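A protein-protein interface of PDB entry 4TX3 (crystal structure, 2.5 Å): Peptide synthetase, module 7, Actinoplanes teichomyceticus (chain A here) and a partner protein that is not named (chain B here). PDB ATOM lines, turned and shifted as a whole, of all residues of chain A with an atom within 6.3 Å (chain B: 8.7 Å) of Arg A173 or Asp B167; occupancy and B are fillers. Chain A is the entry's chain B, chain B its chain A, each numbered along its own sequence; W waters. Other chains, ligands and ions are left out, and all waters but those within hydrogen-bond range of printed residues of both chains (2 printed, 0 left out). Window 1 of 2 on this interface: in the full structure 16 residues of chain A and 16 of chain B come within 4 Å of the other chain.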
ATOM      1  N   ARG A  66      39.798  16.292  16.401  1.00  0.00           N
ATOM      2  CA  ARG A  66      39.605  17.110  17.593  1.00  0.00           C
ATOM      3  C   ARG A  66      40.934  17.647  18.140  1.00  0.00           C
ATOM      4  O   ARG A  66      41.002  18.805  18.557  1.00  0.00           O
ATOM      5  CB  ARG A  66      38.866  16.284  18.653  1.00  0.00           C
ATOM      6  CG  ARG A  66      38.593  16.956  19.988  1.00  0.00           C
ATOM      7  CD  ARG A  66      37.647  16.071  20.805  1.00  0.00           C
ATOM      8  NE  ARG A  66      37.605  16.435  22.217  1.00  0.00           N
ATOM      9  CZ  ARG A  66      36.854  17.415  22.717  1.00  0.00           C
ATOM     10  NH1 ARG A  66      36.068  18.137  21.920  1.00  0.00           N
ATOM     11  NH2 ARG A  66      36.883  17.669  24.019  1.00  0.00           N
ATOM     12  N   ARG A 156      38.330   8.706  26.207  1.00  0.00           N
ATOM     13  CA  ARG A 156      37.065   9.393  26.463  1.00  0.00           C
ATOM     14  C   ARG A 156      36.584   9.986  25.155  1.00  0.00           C
ATOM     15  O   ARG A 156      35.390   9.982  24.870  1.00  0.00           O
ATOM     16  CB  ARG A 156      37.194  10.473  27.551  1.00  0.00           C
ATOM     17  CG  ARG A 156      36.857   9.954  28.980  1.00  0.00           C
ATOM     18  CD  ARG A 156      37.491  10.803  30.084  1.00  0.00           C
ATOM     19  NE  ARG A 156      37.566  12.208  29.678  1.00  0.00           N
ATOM     20  CZ  ARG A 156      38.427  13.090  30.181  1.00  0.00           C
ATOM     21  NH1 ARG A 156      39.297  12.713  31.113  1.00  0.00           N
ATOM     22  NH2 ARG A 156      38.419  14.344  29.751  1.00  0.00           N
ATOM     23  N   ASP A 157      37.509  10.462  24.330  1.00  0.00           N
ATOM     24  CA  ASP A 157      37.102  11.096  23.081  1.00  0.00           C
ATOM     25  C   ASP A 157      36.799  10.065  21.986  1.00  0.00           C
ATOM     26  O   ASP A 157      35.940  10.298  21.134  1.00  0.00           O
ATOM     27  CB  ASP A 157      38.161  12.095  22.630  1.00  0.00           C
ATOM     28  CG  ASP A 157      38.149  13.375  23.479  1.00  0.00           C
ATOM     29  OD1 ASP A 157      37.138  13.613  24.188  1.00  0.00           O
ATOM     30  OD2 ASP A 157      39.143  14.142  23.441  1.00  0.00           O
ATOM     31  N   ALA A 160      33.151   8.839  22.713  1.00  0.00           N
ATOM     32  CA  ALA A 160      32.191   9.852  22.269  1.00  0.00           C
ATOM     33  C   ALA A 160      31.992   9.815  20.751  1.00  0.00           C
ATOM     34  O   ALA A 160      30.856   9.872  20.258  1.00  0.00           O
ATOM     35  CB  ALA A 160      32.639  11.243  22.703  1.00  0.00           C
ATOM     36  N   ALA A 161      33.095   9.703  20.014  1.00  0.00           N
ATOM     37  CA  ALA A 161      33.027   9.674  18.562  1.00  0.00           C
ATOM     38  C   ALA A 161      32.491   8.330  18.037  1.00  0.00           C
ATOM     39  O   ALA A 161      31.756   8.309  17.043  1.00  0.00           O
ATOM     40  CB  ALA A 161      34.378   9.974  17.969  1.00  0.00           C
ATOM     41  N   GLY A 163      30.286   6.404  19.560  1.00  0.00           N
ATOM     42  CA  GLY A 163      28.865   6.523  19.798  1.00  0.00           C
ATOM     43  C   GLY A 163      28.140   7.131  18.615  1.00  0.00           C
ATOM     44  O   GLY A 163      27.212   6.525  18.071  1.00  0.00           O
ATOM     45  N   ALA A 164      28.578   8.316  18.198  1.00  0.00           N
ATOM     46  CA  ALA A 164      27.947   9.041  17.090  1.00  0.00           C
ATOM     47  C   ALA A 164      28.093   8.328  15.748  1.00  0.00           C
ATOM     48  O   ALA A 164      27.105   8.138  15.032  1.00  0.00           O
ATOM     49  CB  ALA A 164      28.523  10.456  16.986  1.00  0.00           C
ATOM     50  N   ARG A 169      25.962   9.415  12.465  1.00  0.00           N
ATOM     51  CA  ARG A 169      26.259  10.844  12.371  1.00  0.00           C
ATOM     52  C   ARG A 169      27.714  11.131  12.758  1.00  0.00           C
ATOM     53  O   ARG A 169      28.335  10.363  13.510  1.00  0.00           O
ATOM     54  CB  ARG A 169      25.311  11.660  13.261  1.00  0.00           C
ATOM     55  CG  ARG A 169      25.630  11.522  14.741  1.00  0.00           C
ATOM     56  CD  ARG A 169      24.779  12.376  15.672  1.00  0.00           C
ATOM     57  NE  ARG A 169      25.230  12.143  17.043  1.00  0.00           N
ATOM     58  CZ  ARG A 169      24.767  11.176  17.830  1.00  0.00           C
ATOM     59  NH1 ARG A 169      23.803  10.368  17.407  1.00  0.00           N
ATOM     60  NH2 ARG A 169      25.259  11.023  19.046  1.00  0.00           N
ATOM     61  N   ALA A 170      28.258  12.225  12.230  1.00  0.00           N
ATOM     62  CA  ALA A 170      29.543  12.751  12.695  1.00  0.00           C
ATOM     63  C   ALA A 170      29.368  13.319  14.119  1.00  0.00           C
ATOM     64  O   ALA A 170      28.264  13.760  14.476  1.00  0.00           O
ATOM     65  CB  ALA A 170      30.068  13.818  11.734  1.00  0.00           C
ATOM     66  N   PRO A 171      30.439  13.295  14.944  1.00  0.00           N
ATOM     67  CA  PRO A 171      30.274  13.757  16.329  1.00  0.00           C
ATOM     68  C   PRO A 171      29.820  15.216  16.383  1.00  0.00           C
ATOM     69  O   PRO A 171      30.304  16.020  15.589  1.00  0.00           O
ATOM     70  CB  PRO A 171      31.676  13.588  16.931  1.00  0.00           C
ATOM     71  CG  PRO A 171      32.396  12.664  16.015  1.00  0.00           C
ATOM     72  CD  PRO A 171      31.834  12.917  14.656  1.00  0.00           C
ATOM     73  N   GLU A 172      28.878  15.532  17.268  1.00  0.00           N
ATOM     74  CA  GLU A 172      28.454  16.915  17.483  1.00  0.00           C
ATOM     75  C   GLU A 172      29.072  17.437  18.776  1.00  0.00           C
ATOM     76  O   GLU A 172      28.540  17.198  19.860  1.00  0.00           O
ATOM     77  CB  GLU A 172      26.927  17.017  17.542  1.00  0.00           C
ATOM     78  CG  GLU A 172      26.224  16.598  16.254  1.00  0.00           C
ATOM     79  CD  GLU A 172      24.702  16.435  16.408  1.00  0.00           C
ATOM     80  OE1 GLU A 172      24.255  15.526  17.146  1.00  0.00           O
ATOM     81  OE2 GLU A 172      23.948  17.204  15.771  1.00  0.00           O
ATOM     82  N   ARG A 173      30.213  18.120  18.669  1.00  0.00           N
ATOM     83  CA  ARG A 173      30.891  18.637  19.858  1.00  0.00           C
ATOM     84  C   ARG A 173      31.385  20.046  19.646  1.00  0.00           C
ATOM     85  O   ARG A 173      31.730  20.419  18.531  1.00  0.00           O
ATOM     86  CB  ARG A 173      32.091  17.765  20.257  1.00  0.00           C
ATOM     87  CG  ARG A 173      31.877  16.266  20.119  1.00  0.00           C
ATOM     88  CD  ARG A 173      32.924  15.497  20.891  1.00  0.00           C
ATOM     89  NE  ARG A 173      32.885  15.834  22.306  1.00  0.00           N
ATOM     90  CZ  ARG A 173      33.790  15.440  23.193  1.00  0.00           C
ATOM     91  NH1 ARG A 173      34.824  14.701  22.819  1.00  0.00           N
ATOM     92  NH2 ARG A 173      33.663  15.798  24.455  1.00  0.00           N
ATOM     93  N   ALA A 174      31.441  20.812  20.731  1.00  0.00           N
ATOM     94  CA  ALA A 174      32.211  22.053  20.769  1.00  0.00           C
ATOM     95  C   ALA A 174      33.711  21.761  20.604  1.00  0.00           C
ATOM     96  O   ALA A 174      34.237  20.817  21.196  1.00  0.00           O
ATOM     97  CB  ALA A 174      31.956  22.791  22.080  1.00  0.00           C
ATOM     98  N   PRO A 175      34.405  22.578  19.805  1.00  0.00           N
ATOM     99  CA  PRO A 175      35.864  22.463  19.627  1.00  0.00           C
ATOM    100  C   PRO A 175      36.635  22.731  20.915  1.00  0.00           C
ATOM    101  O   PRO A 175      36.090  23.378  21.812  1.00  0.00           O
ATOM    102  CB  PRO A 175      36.173  23.536  18.585  1.00  0.00           C
ATOM    103  CG  PRO A 175      35.049  24.524  18.702  1.00  0.00           C
ATOM    104  CD  PRO A 175      33.837  23.723  19.074  1.00  0.00           C
ATOM    105  N   ARG B 124      13.390  11.878  22.764  1.00  0.00           N
ATOM    106  CA  ARG B 124      14.795  11.934  23.092  1.00  0.00           C
ATOM    107  C   ARG B 124      15.039  11.338  24.482  1.00  0.00           C
ATOM    108  O   ARG B 124      16.062  10.700  24.725  1.00  0.00           O
ATOM    109  CB  ARG B 124      15.276  13.369  22.999  1.00  0.00           C
ATOM    110  CG  ARG B 124      16.717  13.529  23.298  1.00  0.00           C
ATOM    111  CD  ARG B 124      17.662  12.888  22.281  1.00  0.00           C
ATOM    112  NE  ARG B 124      19.016  12.963  22.824  1.00  0.00           N
ATOM    113  CZ  ARG B 124      19.775  11.912  23.108  1.00  0.00           C
ATOM    114  NH1 ARG B 124      19.327  10.688  22.851  1.00  0.00           N
ATOM    115  NH2 ARG B 124      20.989  12.088  23.629  1.00  0.00           N
ATOM    116  N   CYS B 159      20.672  17.639  29.961  1.00  0.00           N
ATOM    117  CA  CYS B 159      21.483  18.165  28.858  1.00  0.00           C
ATOM    118  C   CYS B 159      20.620  18.466  27.642  1.00  0.00           C
ATOM    119  O   CYS B 159      20.883  19.427  26.897  1.00  0.00           O
ATOM    120  CB  CYS B 159      22.595  17.199  28.466  1.00  0.00           C
ATOM    121  SG  CYS B 159      23.884  17.025  29.704  1.00  0.00           S
ATOM    122  N   GLU B 160      19.591  17.650  27.444  1.00  0.00           N
ATOM    123  CA  GLU B 160      18.691  17.845  26.314  1.00  0.00           C
ATOM    124  C   GLU B 160      17.777  19.038  26.532  1.00  0.00           C
ATOM    125  O   GLU B 160      17.520  19.819  25.613  1.00  0.00           O
ATOM    126  CB  GLU B 160      17.865  16.591  26.077  1.00  0.00           C
ATOM    127  CG  GLU B 160      18.632  15.553  25.332  1.00  0.00           C
ATOM    128  CD  GLU B 160      18.756  15.905  23.869  1.00  0.00           C
ATOM    129  OE1 GLU B 160      19.784  15.556  23.251  1.00  0.00           O
ATOM    130  OE2 GLU B 160      17.803  16.513  23.334  1.00  0.00           O
ATOM    131  N   GLY B 163      19.964  22.009  25.969  1.00  0.00           N
ATOM    132  CA  GLY B 163      20.448  21.975  24.603  1.00  0.00           C
ATOM    133  C   GLY B 163      21.944  21.768  24.418  1.00  0.00           C
ATOM    134  O   GLY B 163      22.512  22.202  23.425  1.00  0.00           O
ATOM    135  N   VAL B 164      22.586  21.123  25.379  1.00  0.00           N
ATOM    136  CA  VAL B 164      23.990  20.761  25.253  1.00  0.00           C
ATOM    137  C   VAL B 164      24.204  19.872  24.017  1.00  0.00           C
ATOM    138  O   VAL B 164      23.437  18.933  23.784  1.00  0.00           O
ATOM    139  CB  VAL B 164      24.486  20.036  26.515  1.00  0.00           C
ATOM    140  CG1 VAL B 164      25.941  19.651  26.370  1.00  0.00           C
ATOM    141  CG2 VAL B 164      24.240  20.899  27.744  1.00  0.00           C
ATOM    142  N   PRO B 165      25.217  20.205  23.195  1.00  0.00           N
ATOM    143  CA  PRO B 165      25.529  19.400  22.012  1.00  0.00           C
ATOM    144  C   PRO B 165      25.590  17.929  22.340  1.00  0.00           C
ATOM    145  O   PRO B 165      26.128  17.540  23.384  1.00  0.00           O
ATOM    146  CB  PRO B 165      26.884  19.942  21.581  1.00  0.00           C
ATOM    147  CG  PRO B 165      26.761  21.404  21.908  1.00  0.00           C
ATOM    148  CD  PRO B 165      25.991  21.460  23.210  1.00  0.00           C
ATOM    149  N   ARG B 166      25.015  17.134  21.446  1.00  0.00           N
ATOM    150  CA  ARG B 166      24.725  15.737  21.708  1.00  0.00           C
ATOM    151  C   ARG B 166      25.911  14.980  22.261  1.00  0.00           C
ATOM    152  O   ARG B 166      25.812  14.330  23.291  1.00  0.00           O
ATOM    153  CB  ARG B 166      24.239  15.061  20.428  1.00  0.00           C
ATOM    154  CG  ARG B 166      23.628  13.719  20.670  1.00  0.00           C
ATOM    155  CD  ARG B 166      22.240  13.677  20.082  1.00  0.00           C
ATOM    156  NE  ARG B 166      21.699  12.322  20.052  1.00  0.00           N
ATOM    157  CZ  ARG B 166      20.620  11.981  19.360  1.00  0.00           C
ATOM    158  NH1 ARG B 166      19.983  12.907  18.650  1.00  0.00           N
ATOM    159  NH2 ARG B 166      20.183  10.724  19.372  1.00  0.00           N
ATOM    160  N   ASP B 167      27.045  15.096  21.585  1.00  0.00           N
ATOM    161  CA  ASP B 167      28.184  14.256  21.910  1.00  0.00           C
ATOM    162  C   ASP B 167      29.172  14.912  22.885  1.00  0.00           C
ATOM    163  O   ASP B 167      30.267  14.395  23.139  1.00  0.00           O
ATOM    164  CB  ASP B 167      28.855  13.823  20.608  1.00  0.00           C
ATOM    165  CG  ASP B 167      27.910  12.995  19.730  1.00  0.00           C
ATOM    166  OD1 ASP B 167      27.490  11.900  20.189  1.00  0.00           O
ATOM    167  OD2 ASP B 167      27.584  13.436  18.603  1.00  0.00           O
ATOM    168  N   ASP B 168      28.747  16.017  23.479  1.00  0.00           N
ATOM    169  CA  ASP B 168      29.471  16.586  24.608  1.00  0.00           C
ATOM    170  C   ASP B 168      28.791  16.258  25.939  1.00  0.00           C
ATOM    171  O   ASP B 168      29.340  16.536  26.998  1.00  0.00           O
ATOM    172  CB  ASP B 168      29.609  18.111  24.462  1.00  0.00           C
ATOM    173  CG  ASP B 168      30.767  18.527  23.555  1.00  0.00           C
ATOM    174  OD1 ASP B 168      31.796  17.812  23.497  1.00  0.00           O
ATOM    175  OD2 ASP B 168      30.649  19.589  22.903  1.00  0.00           O
ATOM    176  N   GLN B 169      27.606  15.662  25.892  1.00  0.00           N
ATOM    177  CA  GLN B 169      26.794  15.493  27.108  1.00  0.00           C
ATOM    178  C   GLN B 169      27.449  14.610  28.182  1.00  0.00           C
ATOM    179  O   GLN B 169      27.403  14.950  29.365  1.00  0.00           O
ATOM    180  CB  GLN B 169      25.413  14.962  26.740  1.00  0.00           C
ATOM    181  CG  GLN B 169      24.614  15.949  25.857  1.00  0.00           C
ATOM    182  CD  GLN B 169      23.230  15.431  25.496  1.00  0.00           C
ATOM    183  OE1 GLN B 169      22.880  14.311  25.852  1.00  0.00           O
ATOM    184  NE2 GLN B 169      22.438  16.248  24.788  1.00  0.00           N
ATOM    185  N   ALA B 170      28.091  13.515  27.782  1.00  0.00           N
ATOM    186  CA  ALA B 170      28.871  12.727  28.730  1.00  0.00           C
ATOM    187  C   ALA B 170      29.980  13.569  29.385  1.00  0.00           C
ATOM    188  O   ALA B 170      30.140  13.546  30.605  1.00  0.00           O
ATOM    189  CB  ALA B 170      29.456  11.514  28.050  1.00  0.00           C
ATOM    190  N   MET B 171      30.729  14.322  28.577  1.00  0.00           N
ATOM    191  CA  MET B 171      31.783  15.212  29.086  1.00  0.00           C
ATOM    192  C   MET B 171      31.225  16.224  30.074  1.00  0.00           C
ATOM    193  O   MET B 171      31.674  16.325  31.222  1.00  0.00           O
ATOM    194  CB  MET B 171      32.470  15.955  27.938  1.00  0.00           C
ATOM    195  CG  MET B 171      33.484  17.008  28.393  1.00  0.00           C
ATOM    196  SD  MET B 171      34.174  17.965  27.017  1.00  0.00           S
ATOM    197  CE  MET B 171      32.908  19.209  26.761  1.00  0.00           C
ATOM    198  N   PHE B 172      30.227  16.962  29.599  1.00  0.00           N
ATOM    199  CA  PHE B 172      29.563  18.005  30.367  1.00  0.00           C
ATOM    200  C   PHE B 172      29.035  17.487  31.715  1.00  0.00           C
ATOM    201  O   PHE B 172      29.244  18.109  32.748  1.00  0.00           O
ATOM    202  CB  PHE B 172      28.438  18.609  29.510  1.00  0.00           C
ATOM    203  CG  PHE B 172      27.654  19.695  30.189  1.00  0.00           C
ATOM    204  CD1 PHE B 172      28.158  20.980  30.278  1.00  0.00           C
ATOM    205  CD2 PHE B 172      26.395  19.431  30.713  1.00  0.00           C
ATOM    206  CE1 PHE B 172      27.435  21.989  30.910  1.00  0.00           C
ATOM    207  CE2 PHE B 172      25.667  20.434  31.343  1.00  0.00           C
ATOM    208  CZ  PHE B 172      26.188  21.715  31.440  1.00  0.00           C
ATOM    209  N   TYR B 199      31.730  26.329  29.815  1.00  0.00           N
ATOM    210  CA  TYR B 199      31.094  25.651  28.705  1.00  0.00           C
ATOM    211  C   TYR B 199      29.758  26.319  28.360  1.00  0.00           C
ATOM    212  O   TYR B 199      29.446  26.541  27.189  1.00  0.00           O
ATOM    213  CB  TYR B 199      30.903  24.165  29.027  1.00  0.00           C
ATOM    214  CG  TYR B 199      30.406  23.370  27.844  1.00  0.00           C
ATOM    215  CD1 TYR B 199      29.050  23.317  27.545  1.00  0.00           C
ATOM    216  CD2 TYR B 199      31.292  22.678  27.021  1.00  0.00           C
ATOM    217  CE1 TYR B 199      28.586  22.603  26.463  1.00  0.00           C
ATOM    218  CE2 TYR B 199      30.837  21.956  25.936  1.00  0.00           C
ATOM    219  CZ  TYR B 199      29.481  21.921  25.660  1.00  0.00           C
ATOM    220  OH  TYR B 199      28.996  21.212  24.580  1.00  0.00           O
ATOM    221  N   ARG B 206      27.116  31.145  21.147  1.00  0.00           N
ATOM    222  CA  ARG B 206      26.648  30.521  19.918  1.00  0.00           C
ATOM    223  C   ARG B 206      25.139  30.680  19.737  1.00  0.00           C
ATOM    224  O   ARG B 206      24.687  31.124  18.680  1.00  0.00           O
ATOM    225  CB  ARG B 206      27.025  29.038  19.895  1.00  0.00           C
ATOM    226  CG  ARG B 206      28.502  28.749  20.139  1.00  0.00           C
ATOM    227  CD  ARG B 206      28.848  27.301  19.775  1.00  0.00           C
ATOM    228  NE  ARG B 206      29.239  26.484  20.930  1.00  0.00           N
ATOM    229  CZ  ARG B 206      28.499  25.502  21.447  1.00  0.00           C
ATOM    230  NH1 ARG B 206      27.316  25.204  20.917  1.00  0.00           N
ATOM    231  NH2 ARG B 206      28.938  24.804  22.494  1.00  0.00           N
HETATM  232  O   HOH W   1      33.641  19.443  23.275  1.00  0.00           O
HETATM  233  O   HOH W   2      28.711  10.437  21.772  1.00  0.00           O
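Of the 14 printed residues of chain A, 7 touch a printed residue of chain B.
Printed residues of chain A that touch a printed residue of chain B: Ala A160, Ala A164, Arg A169, Pro A171, Glu A172, Arg A173 and Ala A174.
Hydrophobic or aromatic side chains of chain A within 4 Å of the printed part of chain B: Ala A160, Ala A164 and Ala A174.
Among the printed residues, Asp or Glu carboxylates within 4 Å of a Lys or Arg side-chain nitrogen of the other chain: Arg A169 with Asp B167 (2.7 Å) and Arg A173 with Asp B168 (2.6 Å).
Arg A173 touches three residues of chain B.
Of chain B, only Asp B168 and Arg B206 come within 4 Å of Ala A174.
Printed residues of chain A within 4 Å of Asp B168: Glu A172, Arg A173 and Ala A174.
Of the printed residues of chain B, Glu A172 touches Pro B165, Arg B166, Asp B167 and Asp B168.
Of the printed residues of chain A, Arg B166 touches Arg A169 (3.5 Å) and Glu A172 (3.3 Å).
Printed residues of chain B within 4 Å of Pro A171: Asp B167 (3.5 Å).
Ala A161 touches none of the printed residues of chain B.
The nearest residue of chain A that does not touch Asp B167 is Ala A170 (4.2 Å).
The nearest printed residue of chain A that does not touch Met B171 is Arg A66 (4.1 Å).
Water W1 lies within hydrogen-bond range of OD1 of Asp B168, O of Ala A174 and NH1 of Arg A66.
Water W2 bridges the side-chain carboxylate (OD1) of Asp B167 (2.5 Å) and the backbone carbonyl oxygen (O) of Ala A160 (2.7 Å).
O of Ala A164 sits at hydrogen-bond distance from N of Arg A169, at 3.1 Å.
The side-chain carboxylate (OD1) of Asp A157 is in salt-bridge range of the guanidinium group (NH1) of Arg A173, at 2.9 Å.
The side-chain carboxylate of Asp B168 is in hydrogen-bond range of the side-chain hydroxyl of Tyr B199, 2.9 Å away.
OE1 of Glu A172 is in salt-bridge range of NE of Arg A169, at 3.5 Å.
The guanidinium group (NH1) of Arg A66 sits at hydrogen-bond distance from the backbone carbonyl oxygen (O) of Ala A174, 3.3 Å away.
The guanidinium group (NH2) of Arg A169 is in salt-bridge range of the side-chain carboxylate (OD1) of Asp B167 (2.7 Å).
The guanidinium group (NE) of Arg A173 sits at hydrogen-bond distance from the backbone carbonyl oxygen (O) of Asp B167 (3.1 Å).
OD2 of Asp B167 lies within hydrogen-bond range of N of Glu A172 (2.8 Å).
The guanidinium group (NH2) of Arg A173 lies within hydrogen-bond range of the side-chain sulfur (SD) of Met B171 (3.4 Å).
The side-chain carboxylate (OD1) of Asp B168 lies within salt-bridge range of the guanidinium group (NE) of Arg A173 (2.6 Å).
OD2 of Asp B168 sits at hydrogen-bond distance from N of Ala A174 (2.6 Å).
OD1 of Asp B167 touches O of Ala A160, 3.9 Å away.
Ala A164 touches Asp B167 (CB to OD2, 3.5 Å).
Arg A169 touches Arg B166 (NH2 to CG, 3.5 Å).
Asp B167 touches Pro A171 (OD2 to CA, 3.5 Å).
Glu A172 touches Pro B165.
OE1 of Glu A172 touches CB of Arg B166, at 3.3 Å.
Asp B168 touches Glu A172 (N to O, 3.8 Å).
Arg B206 touches Ala A174 (NH2 to CB, 3.7 Å).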
